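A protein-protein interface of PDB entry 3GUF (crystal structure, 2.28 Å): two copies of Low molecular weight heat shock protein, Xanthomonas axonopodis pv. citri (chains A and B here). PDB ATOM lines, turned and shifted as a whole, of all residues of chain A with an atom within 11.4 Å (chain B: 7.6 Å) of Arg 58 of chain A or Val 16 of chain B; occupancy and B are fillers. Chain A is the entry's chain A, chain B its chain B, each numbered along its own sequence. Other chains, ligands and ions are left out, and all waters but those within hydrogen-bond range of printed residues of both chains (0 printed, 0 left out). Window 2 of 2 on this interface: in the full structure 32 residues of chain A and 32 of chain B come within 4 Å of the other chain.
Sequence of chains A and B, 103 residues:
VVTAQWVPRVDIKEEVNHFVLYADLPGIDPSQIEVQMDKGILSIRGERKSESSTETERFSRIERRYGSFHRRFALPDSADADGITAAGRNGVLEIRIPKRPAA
The side-chain carboxylate of Glu 55 of chain A is in salt-bridge range of the guanidinium group of Arg 58 of chain A (3.7 Å).
The side-chain carboxylate (OE1) of Glu 15 of chain B lies within salt-bridge range of the side-chain amino group (NZ) of Lys 13 of chain B (2.8 Å).
The backbone NH of Lys 13 of chain B sits at hydrogen-bond distance from the backbone carbonyl oxygen of Val 20 of chain B (2.7 Å).
NZ of Lys 99 of chain B lies within salt-bridge range of OE2 of Glu 14 of chain B (3.5 Å).
NZ of Lys 99 of chain B sits at hydrogen-bond distance from O of Glu 15 of chain B (3.0 Å).
NZ of Lys 99 of chain B lies within hydrogen-bond range of O of Val 16 of chain B (3.1 Å).
No position is printed for both chains.
Among the printed residues, pairs that only touch across the chains: Glu 55 of chain A with Glu 15 of chain B (3.9 Å), Arg 58 of chain A with Lys 13 of chain B (3.5 Å), Arg 58 of chain A with Glu 15 of chain B (3.5 Å), Arg 58 of chain A with Val 16 of chain B (3.6 Å), Phe 59 of chain A with Ile 12 of chain B (3.4 Å) and Phe 59 of chain A with Lys 13 of chain B (3.3 Å).
Arg 58 of chain A touches just these residues of chain B: Lys 13, Glu 14, Glu 15 and Val 16.
Of the printed residues of chain A, Val 16 of chain B touches Arg 58 (3.6 Å).
Printed residues of chain A within 4 Å of Lys 13 of chain B: Glu 55, Arg 58 and Phe 59.
Glu 14 of chain B touches just one residue of chain A: Arg 58 (2.8 Å).
Asn 17 of chain B touches none of the printed residues of chain A.
Of the printed residues of chain B, Phe 59 of chain A touches Ile 12 and Lys 13.
Printed residues of chain B within 4 Å of Arg 61 of chain A: Ile 12 (2.6 Å).
Of the printed residues of chain B, Ser 60 of chain A touches Ile 12 (2.7 Å).
Printed residues of chain B within 4 Å of Glu 55 of chain A: Lys 13 and Glu 15.
Val 20 of chain B touches none of the printed residues of chain A.
Glu 57 of chain A touches none of the printed residues of chain B.
The nearest residue of chain A that does not touch Val 16 of chain B is Glu 55 of chain A (6.0 Å).
The side-chain carboxylate of Glu 55 of chain A is in salt-bridge range of the side-chain amino group of Lys 13 of chain B (3.6 Å).
O of Arg 58 of chain A sits at hydrogen-bond distance from N of Glu 14 of chain B (2.8 Å).
The backbone NH of Ser 60 of chain A lies within hydrogen-bond range of the backbone carbonyl oxygen of Ile 12 of chain B, 2.7 Å away.
O of Arg 61 of chain A lies within hydrogen-bond range of N of Ile 12 of chain B (2.6 Å).
Printed residues of chain B that touch a printed residue of chain A: Ile 12, Lys 13, Glu 14, Glu 15 and Val 16.
Hydrophobic or aromatic side chains of chain B within 4 Å of the printed part of chain A: Ile 12 and Val 16.
Of the 13 printed residues of chain A, 5 touch a printed residue of chain B.
Among the printed residues, 10 pairs touch across the chains.
Among the printed residues, Asp or Glu carboxylates within 4 Å of a Lys or Arg side-chain nitrogen of the other chain: Glu 55 of chain A with Lys 13 of chain B (3.6 Å).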
ATOM      1  N   GLU A  51      27.326 -34.396  18.838  1.00  0.00           N
ATOM      2  CA  GLU A  51      27.409 -33.058  18.256  1.00  0.00           C
ATOM      3  C   GLU A  51      26.086 -32.335  18.474  1.00  0.00           C
ATOM      4  O   GLU A  51      25.919 -31.189  18.032  1.00  0.00           O
ATOM      5  CB  GLU A  51      27.732 -33.124  16.760  1.00  0.00           C
ATOM      6  CG  GLU A  51      28.750 -34.201  16.368  1.00  0.00           C
ATOM      7  CD  GLU A  51      28.116 -35.577  16.084  1.00  0.00           C
ATOM      8  OE1 GLU A  51      26.953 -35.843  16.491  1.00  0.00           O
ATOM      9  OE2 GLU A  51      28.788 -36.397  15.434  1.00  0.00           O
ATOM     10  N   SER A  52      25.148 -33.002  19.157  1.00  0.00           N
ATOM     11  CA  SER A  52      23.919 -32.337  19.595  1.00  0.00           C
ATOM     12  C   SER A  52      24.161 -31.469  20.842  1.00  0.00           C
ATOM     13  O   SER A  52      23.279 -30.717  21.261  1.00  0.00           O
ATOM     14  CB  SER A  52      22.753 -33.322  19.777  1.00  0.00           C
ATOM     15  OG  SER A  52      22.431 -33.524  21.135  1.00  0.00           O
ATOM     16  N   SER A  53      25.360 -31.583  21.421  1.00  0.00           N
ATOM     17  CA  SER A  53      25.783 -30.717  22.529  1.00  0.00           C
ATOM     18  C   SER A  53      26.395 -29.400  22.001  1.00  0.00           C
ATOM     19  O   SER A  53      26.175 -28.326  22.571  1.00  0.00           O
ATOM     20  CB  SER A  53      26.732 -31.457  23.501  1.00  0.00           C
ATOM     21  OG  SER A  53      27.905 -31.964  22.873  1.00  0.00           O
ATOM     22  N   THR A  54      27.141 -29.505  20.900  1.00  0.00           N
ATOM     23  CA  THR A  54      27.760 -28.353  20.221  1.00  0.00           C
ATOM     24  C   THR A  54      26.766 -27.662  19.286  1.00  0.00           C
ATOM     25  O   THR A  54      26.351 -28.243  18.275  1.00  0.00           O
ATOM     26  CB  THR A  54      29.034 -28.779  19.418  1.00  0.00           C
ATOM     27  OG1 THR A  54      29.989 -29.377  20.307  1.00  0.00           O
ATOM     28  CG2 THR A  54      29.688 -27.577  18.731  1.00  0.00           C
ATOM     29  N   GLU A  55      26.401 -26.425  19.637  1.00  0.00           N
ATOM     30  CA  GLU A  55      25.475 -25.579  18.852  1.00  0.00           C
ATOM     31  C   GLU A  55      24.030 -26.110  18.884  1.00  0.00           C
ATOM     32  O   GLU A  55      23.405 -26.290  17.848  1.00  0.00           O
ATOM     33  CB  GLU A  55      25.984 -25.371  17.403  1.00  0.00           C
ATOM     34  CG  GLU A  55      27.312 -24.589  17.275  1.00  0.00           C
ATOM     35  CD  GLU A  55      27.960 -24.634  15.866  1.00  0.00           C
ATOM     36  OE1 GLU A  55      27.233 -24.597  14.837  1.00  0.00           O
ATOM     37  OE2 GLU A  55      29.216 -24.685  15.791  1.00  0.00           O
ATOM     38  N   THR A  56      23.507 -26.320  20.090  1.00  0.00           N
ATOM     39  CA  THR A  56      22.265 -27.083  20.312  1.00  0.00           C
ATOM     40  C   THR A  56      20.956 -26.426  19.812  1.00  0.00           C
ATOM     41  O   THR A  56      20.067 -27.115  19.280  1.00  0.00           O
ATOM     42  CB  THR A  56      22.144 -27.493  21.806  1.00  0.00           C
ATOM     43  OG1 THR A  56      23.343 -28.157  22.202  1.00  0.00           O
ATOM     44  CG2 THR A  56      20.961 -28.423  22.058  1.00  0.00           C
ATOM     45  N   GLU A  57      20.831 -25.108  20.001  1.00  0.00           N
ATOM     46  CA  GLU A  57      19.725 -24.305  19.416  1.00  0.00           C
ATOM     47  C   GLU A  57      19.451 -24.634  17.933  1.00  0.00           C
ATOM     48  O   GLU A  57      18.312 -24.583  17.478  1.00  0.00           O
ATOM     49  CB  GLU A  57      19.998 -22.798  19.588  1.00  0.00           C
ATOM     50  CG  GLU A  57      21.357 -22.295  19.021  1.00  0.00           C
ATOM     51  CD  GLU A  57      22.591 -22.720  19.858  1.00  0.00           C
ATOM     52  OE1 GLU A  57      23.718 -22.795  19.298  1.00  0.00           O
ATOM     53  OE2 GLU A  57      22.426 -22.977  21.079  1.00  0.00           O
ATOM     54  N   ARG A  58      20.514 -24.987  17.209  1.00  0.00           N
ATOM     55  CA  ARG A  58      20.461 -25.340  15.779  1.00  0.00           C
ATOM     56  C   ARG A  58      19.796 -26.696  15.434  1.00  0.00           C
ATOM     57  O   ARG A  58      19.617 -27.013  14.255  1.00  0.00           O
ATOM     58  CB  ARG A  58      21.877 -25.314  15.161  1.00  0.00           C
ATOM     59  CG  ARG A  58      22.671 -24.025  15.380  1.00  0.00           C
ATOM     60  CD  ARG A  58      24.009 -24.036  14.606  1.00  0.00           C
ATOM     61  NE  ARG A  58      24.124 -23.173  13.409  1.00  0.00           N
ATOM     62  CZ  ARG A  58      23.126 -22.597  12.723  1.00  0.00           C
ATOM     63  NH1 ARG A  58      21.846 -22.758  13.072  1.00  0.00           N
ATOM     64  NH2 ARG A  58      23.413 -21.853  11.651  1.00  0.00           N
ATOM     65  N   PHE A  59      19.438 -27.487  16.444  1.00  0.00           N
ATOM     66  CA  PHE A  59      18.885 -28.824  16.219  1.00  0.00           C
ATOM     67  C   PHE A  59      17.336 -28.872  16.153  1.00  0.00           C
ATOM     68  O   PHE A  59      16.627 -28.588  17.121  1.00  0.00           O
ATOM     69  CB  PHE A  59      19.441 -29.803  17.262  1.00  0.00           C
ATOM     70  CG  PHE A  59      20.853 -30.255  16.986  1.00  0.00           C
ATOM     71  CD1 PHE A  59      21.929 -29.369  17.121  1.00  0.00           C
ATOM     72  CD2 PHE A  59      21.111 -31.578  16.597  1.00  0.00           C
ATOM     73  CE1 PHE A  59      23.233 -29.787  16.879  1.00  0.00           C
ATOM     74  CE2 PHE A  59      22.412 -31.998  16.330  1.00  0.00           C
ATOM     75  CZ  PHE A  59      23.472 -31.108  16.475  1.00  0.00           C
ATOM     76  N   SER A  60      16.830 -29.252  14.997  1.00  0.00           N
ATOM     77  CA  SER A  60      15.406 -29.278  14.768  1.00  0.00           C
ATOM     78  C   SER A  60      14.777 -30.592  15.201  1.00  0.00           C
ATOM     79  O   SER A  60      13.554 -30.729  15.202  1.00  0.00           O
ATOM     80  CB  SER A  60      15.133 -29.022  13.283  1.00  0.00           C
ATOM     81  OG  SER A  60      16.201 -29.490  12.450  1.00  0.00           O
ATOM     82  N   ARG A  61      15.622 -31.573  15.532  1.00  0.00           N
ATOM     83  CA  ARG A  61      15.181 -32.922  15.945  1.00  0.00           C
ATOM     84  C   ARG A  61      16.361 -33.674  16.530  1.00  0.00           C
ATOM     85  O   ARG A  61      17.409 -33.765  15.909  1.00  0.00           O
ATOM     86  CB  ARG A  61      14.474 -33.693  14.820  1.00  0.00           C
ATOM     87  CG  ARG A  61      15.226 -34.853  14.160  1.00  0.00           C
ATOM     88  CD  ARG A  61      14.281 -36.022  13.842  1.00  0.00           C
ATOM     89  NE  ARG A  61      12.926 -35.578  13.559  1.00  0.00           N
ATOM     90  CZ  ARG A  61      11.827 -36.330  13.614  1.00  0.00           C
ATOM     91  NH1 ARG A  61      11.880 -37.615  13.921  1.00  0.00           N
ATOM     92  NH2 ARG A  61      10.645 -35.776  13.343  1.00  0.00           N
ATOM     93  N   ILE A  62      16.190 -34.128  17.770  1.00  0.00           N
ATOM     94  CA  ILE A  62      17.247 -34.813  18.524  1.00  0.00           C
ATOM     95  C   ILE A  62      16.580 -36.058  19.059  1.00  0.00           C
ATOM     96  O   ILE A  62      15.740 -35.969  19.965  1.00  0.00           O
ATOM     97  CB  ILE A  62      17.827 -33.957  19.690  1.00  0.00           C
ATOM     98  CG1 ILE A  62      18.765 -32.853  19.174  1.00  0.00           C
ATOM     99  CG2 ILE A  62      18.596 -34.812  20.665  1.00  0.00           C
ATOM    100  CD1 ILE A  62      19.261 -31.827  20.284  1.00  0.00           C
ATOM    101  N   GLU A  63      16.908 -37.210  18.463  1.00  0.00           N
ATOM    102  CA  GLU A  63      16.347 -38.480  18.914  1.00  0.00           C
ATOM    103  C   GLU A  63      17.450 -39.252  19.597  1.00  0.00           C
ATOM    104  O   GLU A  63      17.191 -40.139  20.408  1.00  0.00           O
ATOM    105  CB  GLU A  63      15.855 -39.301  17.744  1.00  0.00           C
ATOM    106  CG  GLU A  63      14.863 -38.630  16.831  1.00  0.00           C
ATOM    107  CD  GLU A  63      14.303 -39.579  15.792  1.00  0.00           C
ATOM    108  OE1 GLU A  63      14.987 -40.577  15.424  1.00  0.00           O
ATOM    109  OE2 GLU A  63      13.167 -39.330  15.334  1.00  0.00           O
ATOM    110  N   ILE B  12      18.551 -34.178  13.609  1.00  0.00           N
ATOM    111  CA  ILE B  12      18.647 -33.188  12.509  1.00  0.00           C
ATOM    112  C   ILE B  12      19.038 -31.764  12.957  1.00  0.00           C
ATOM    113  O   ILE B  12      18.353 -31.148  13.783  1.00  0.00           O
ATOM    114  CB  ILE B  12      17.381 -33.129  11.662  1.00  0.00           C
ATOM    115  CG1 ILE B  12      17.180 -34.440  10.898  1.00  0.00           C
ATOM    116  CG2 ILE B  12      17.511 -31.988  10.600  1.00  0.00           C
ATOM    117  CD1 ILE B  12      15.708 -34.813  10.619  1.00  0.00           C
ATOM    118  N   LYS B  13      20.133 -31.259  12.390  1.00  0.00           N
ATOM    119  CA  LYS B  13      20.739 -29.983  12.741  1.00  0.00           C
ATOM    120  C   LYS B  13      20.665 -29.040  11.503  1.00  0.00           C
ATOM    121  O   LYS B  13      20.891 -29.489  10.369  1.00  0.00           O
ATOM    122  CB  LYS B  13      22.202 -30.233  13.086  1.00  0.00           C
ATOM    123  CG  LYS B  13      22.951 -29.051  13.660  1.00  0.00           C
ATOM    124  CD  LYS B  13      24.458 -29.253  13.640  1.00  0.00           C
ATOM    125  CE  LYS B  13      25.173 -27.962  14.058  1.00  0.00           C
ATOM    126  NZ  LYS B  13      26.679 -27.985  13.832  1.00  0.00           N
ATOM    127  N   GLU B  14      20.348 -27.756  11.695  1.00  0.00           N
ATOM    128  CA  GLU B  14      20.375 -26.788  10.556  1.00  0.00           C
ATOM    129  C   GLU B  14      21.596 -25.943  10.730  1.00  0.00           C
ATOM    130  O   GLU B  14      21.657 -25.125  11.625  1.00  0.00           O
ATOM    131  CB  GLU B  14      19.091 -25.932  10.446  1.00  0.00           C
ATOM    132  CG  GLU B  14      19.144 -24.702   9.461  1.00  0.00           C
ATOM    133  CD  GLU B  14      17.737 -24.209   9.049  1.00  0.00           C
ATOM    134  OE1 GLU B  14      16.762 -24.510   9.776  1.00  0.00           O
ATOM    135  OE2 GLU B  14      17.594 -23.530   7.996  1.00  0.00           O
ATOM    136  N   GLU B  15      22.598 -26.202   9.915  1.00  0.00           N
ATOM    137  CA  GLU B  15      23.871 -25.529  10.049  1.00  0.00           C
ATOM    138  C   GLU B  15      23.842 -24.293   9.175  1.00  0.00           C
ATOM    139  O   GLU B  15      22.811 -23.915   8.632  1.00  0.00           O
ATOM    140  CB  GLU B  15      25.028 -26.428   9.589  1.00  0.00           C
ATOM    141  CG  GLU B  15      25.465 -27.464  10.599  1.00  0.00           C
ATOM    142  CD  GLU B  15      26.970 -27.489  10.781  1.00  0.00           C
ATOM    143  OE1 GLU B  15      27.486 -26.633  11.560  1.00  0.00           O
ATOM    144  OE2 GLU B  15      27.628 -28.365  10.159  1.00  0.00           O
ATOM    145  N   VAL B  16      25.014 -23.693   9.037  1.00  0.00           N
ATOM    146  CA  VAL B  16      25.160 -22.497   8.310  1.00  0.00           C
ATOM    147  C   VAL B  16      24.904 -22.861   6.858  1.00  0.00           C
ATOM    148  O   VAL B  16      23.850 -22.495   6.280  1.00  0.00           O
ATOM    149  CB  VAL B  16      26.544 -21.884   8.581  1.00  0.00           C
ATOM    150  CG1 VAL B  16      26.938 -20.899   7.473  1.00  0.00           C
ATOM    151  CG2 VAL B  16      26.529 -21.203   9.953  1.00  0.00           C
ATOM    152  N   ASN B  17      25.832 -23.615   6.273  1.00  0.00           N
ATOM    153  CA  ASN B  17      25.690 -23.955   4.864  1.00  0.00           C
ATOM    154  C   ASN B  17      24.875 -25.221   4.679  1.00  0.00           C
ATOM    155  O   ASN B  17      24.625 -25.621   3.545  1.00  0.00           O
ATOM    156  CB  ASN B  17      27.058 -24.085   4.186  1.00  0.00           C
ATOM    157  CG  ASN B  17      27.785 -22.748   4.077  1.00  0.00           C
ATOM    158  OD1 ASN B  17      29.023 -22.681   4.194  1.00  0.00           O
ATOM    159  ND2 ASN B  17      27.019 -21.667   3.876  1.00  0.00           N
ATOM    160  N   HIS B  18      24.453 -25.852   5.779  1.00  0.00           N
ATOM    161  CA  HIS B  18      24.033 -27.240   5.684  1.00  0.00           C
ATOM    162  C   HIS B  18      22.851 -27.684   6.557  1.00  0.00           C
ATOM    163  O   HIS B  18      22.555 -27.129   7.605  1.00  0.00           O
ATOM    164  CB  HIS B  18      25.223 -28.142   5.963  1.00  0.00           C
ATOM    165  CG  HIS B  18      26.338 -28.031   4.970  1.00  0.00           C
ATOM    166  ND1 HIS B  18      26.233 -28.495   3.680  1.00  0.00           N
ATOM    167  CD2 HIS B  18      27.610 -27.577   5.103  1.00  0.00           C
ATOM    168  CE1 HIS B  18      27.386 -28.321   3.054  1.00  0.00           C
ATOM    169  NE2 HIS B  18      28.239 -27.766   3.896  1.00  0.00           N
ATOM    170  N   PHE B  19      22.151 -28.693   6.083  1.00  0.00           N
ATOM    171  CA  PHE B  19      21.320 -29.468   6.970  1.00  0.00           C
ATOM    172  C   PHE B  19      22.184 -30.688   7.259  1.00  0.00           C
ATOM    173  O   PHE B  19      22.815 -31.258   6.356  1.00  0.00           O
ATOM    174  CB  PHE B  19      20.002 -29.873   6.333  1.00  0.00           C
ATOM    175  CG  PHE B  19      18.955 -28.804   6.353  1.00  0.00           C
ATOM    176  CD1 PHE B  19      18.600 -28.143   5.178  1.00  0.00           C
ATOM    177  CD2 PHE B  19      18.290 -28.480   7.525  1.00  0.00           C
ATOM    178  CE1 PHE B  19      17.616 -27.142   5.163  1.00  0.00           C
ATOM    179  CE2 PHE B  19      17.276 -27.468   7.529  1.00  0.00           C
ATOM    180  CZ  PHE B  19      16.944 -26.801   6.336  1.00  0.00           C
ATOM    181  N   VAL B  20      22.267 -31.040   8.532  1.00  0.00           N
ATOM    182  CA  VAL B  20      23.003 -32.234   8.917  1.00  0.00           C
ATOM    183  C   VAL B  20      22.083 -33.185   9.622  1.00  0.00           C
ATOM    184  O   VAL B  20      21.415 -32.854  10.607  1.00  0.00           O
ATOM    185  CB  VAL B  20      24.219 -31.936   9.745  1.00  0.00           C
ATOM    186  CG1 VAL B  20      25.177 -33.110   9.613  1.00  0.00           C
ATOM    187  CG2 VAL B  20      24.886 -30.678   9.218  1.00  0.00           C
ATOM    188  N   ARG B  96      24.962 -34.850   5.236  1.00  0.00           N
ATOM    189  CA  ARG B  96      25.124 -33.371   5.074  1.00  0.00           C
ATOM    190  C   ARG B  96      24.451 -32.857   3.788  1.00  0.00           C
ATOM    191  O   ARG B  96      24.891 -33.181   2.687  1.00  0.00           O
ATOM    192  CB  ARG B  96      26.610 -32.990   5.063  1.00  0.00           C
ATOM    193  CG  ARG B  96      27.172 -32.815   6.459  1.00  0.00           C
ATOM    194  CD  ARG B  96      28.569 -32.254   6.448  1.00  0.00           C
ATOM    195  NE  ARG B  96      28.884 -31.715   7.757  1.00  0.00           N
ATOM    196  CZ  ARG B  96      28.886 -30.410   8.084  1.00  0.00           C
ATOM    197  NH1 ARG B  96      29.211 -30.042   9.334  1.00  0.00           N
ATOM    198  NH2 ARG B  96      28.572 -29.457   7.189  1.00  0.00           N
ATOM    199  N   PRO B  98      23.255 -29.653   1.501  1.00  0.00           N
ATOM    200  CA  PRO B  98      23.404 -28.183   1.395  1.00  0.00           C
ATOM    201  C   PRO B  98      22.055 -27.457   1.269  1.00  0.00           C
ATOM    202  O   PRO B  98      21.008 -28.083   1.016  1.00  0.00           O
ATOM    203  CB  PRO B  98      24.276 -27.988   0.144  1.00  0.00           C
ATOM    204  CG  PRO B  98      24.616 -29.360  -0.368  1.00  0.00           C
ATOM    205  CD  PRO B  98      23.579 -30.288   0.217  1.00  0.00           C
ATOM    206  N   LYS B  99      22.053 -26.162   1.524  1.00  0.00           N
ATOM    207  CA  LYS B  99      20.863 -25.374   1.218  1.00  0.00           C
ATOM    208  C   LYS B  99      20.947 -24.855  -0.232  1.00  0.00           C
ATOM    209  O   LYS B  99      22.059 -24.632  -0.757  1.00  0.00           O
ATOM    210  CB  LYS B  99      20.747 -24.225   2.194  1.00  0.00           C
ATOM    211  CG  LYS B  99      20.635 -24.669   3.613  1.00  0.00           C
ATOM    212  CD  LYS B  99      21.057 -23.583   4.540  1.00  0.00           C
ATOM    213  CE  LYS B  99      20.039 -23.418   5.628  1.00  0.00           C
ATOM    214  NZ  LYS B  99      20.788 -22.832   6.739  1.00  0.00           N
ATOM    215  N   PRO B 101      21.408 -22.227  -1.942  1.00  0.00           N
ATOM    216  CA  PRO B 101      21.821 -21.049  -1.130  1.00  0.00           C
ATOM    217  C   PRO B 101      20.750 -20.443  -0.170  1.00  0.00           C
ATOM    218  O   PRO B 101      20.844 -20.560   1.081  1.00  0.00           O
ATOM    219  CB  PRO B 101      22.291 -20.073  -2.205  1.00  0.00           C
ATOM    220  CG  PRO B 101      23.013 -21.026  -3.190  1.00  0.00           C
ATOM    221  CD  PRO B 101      22.431 -22.444  -2.991  1.00  0.00           C
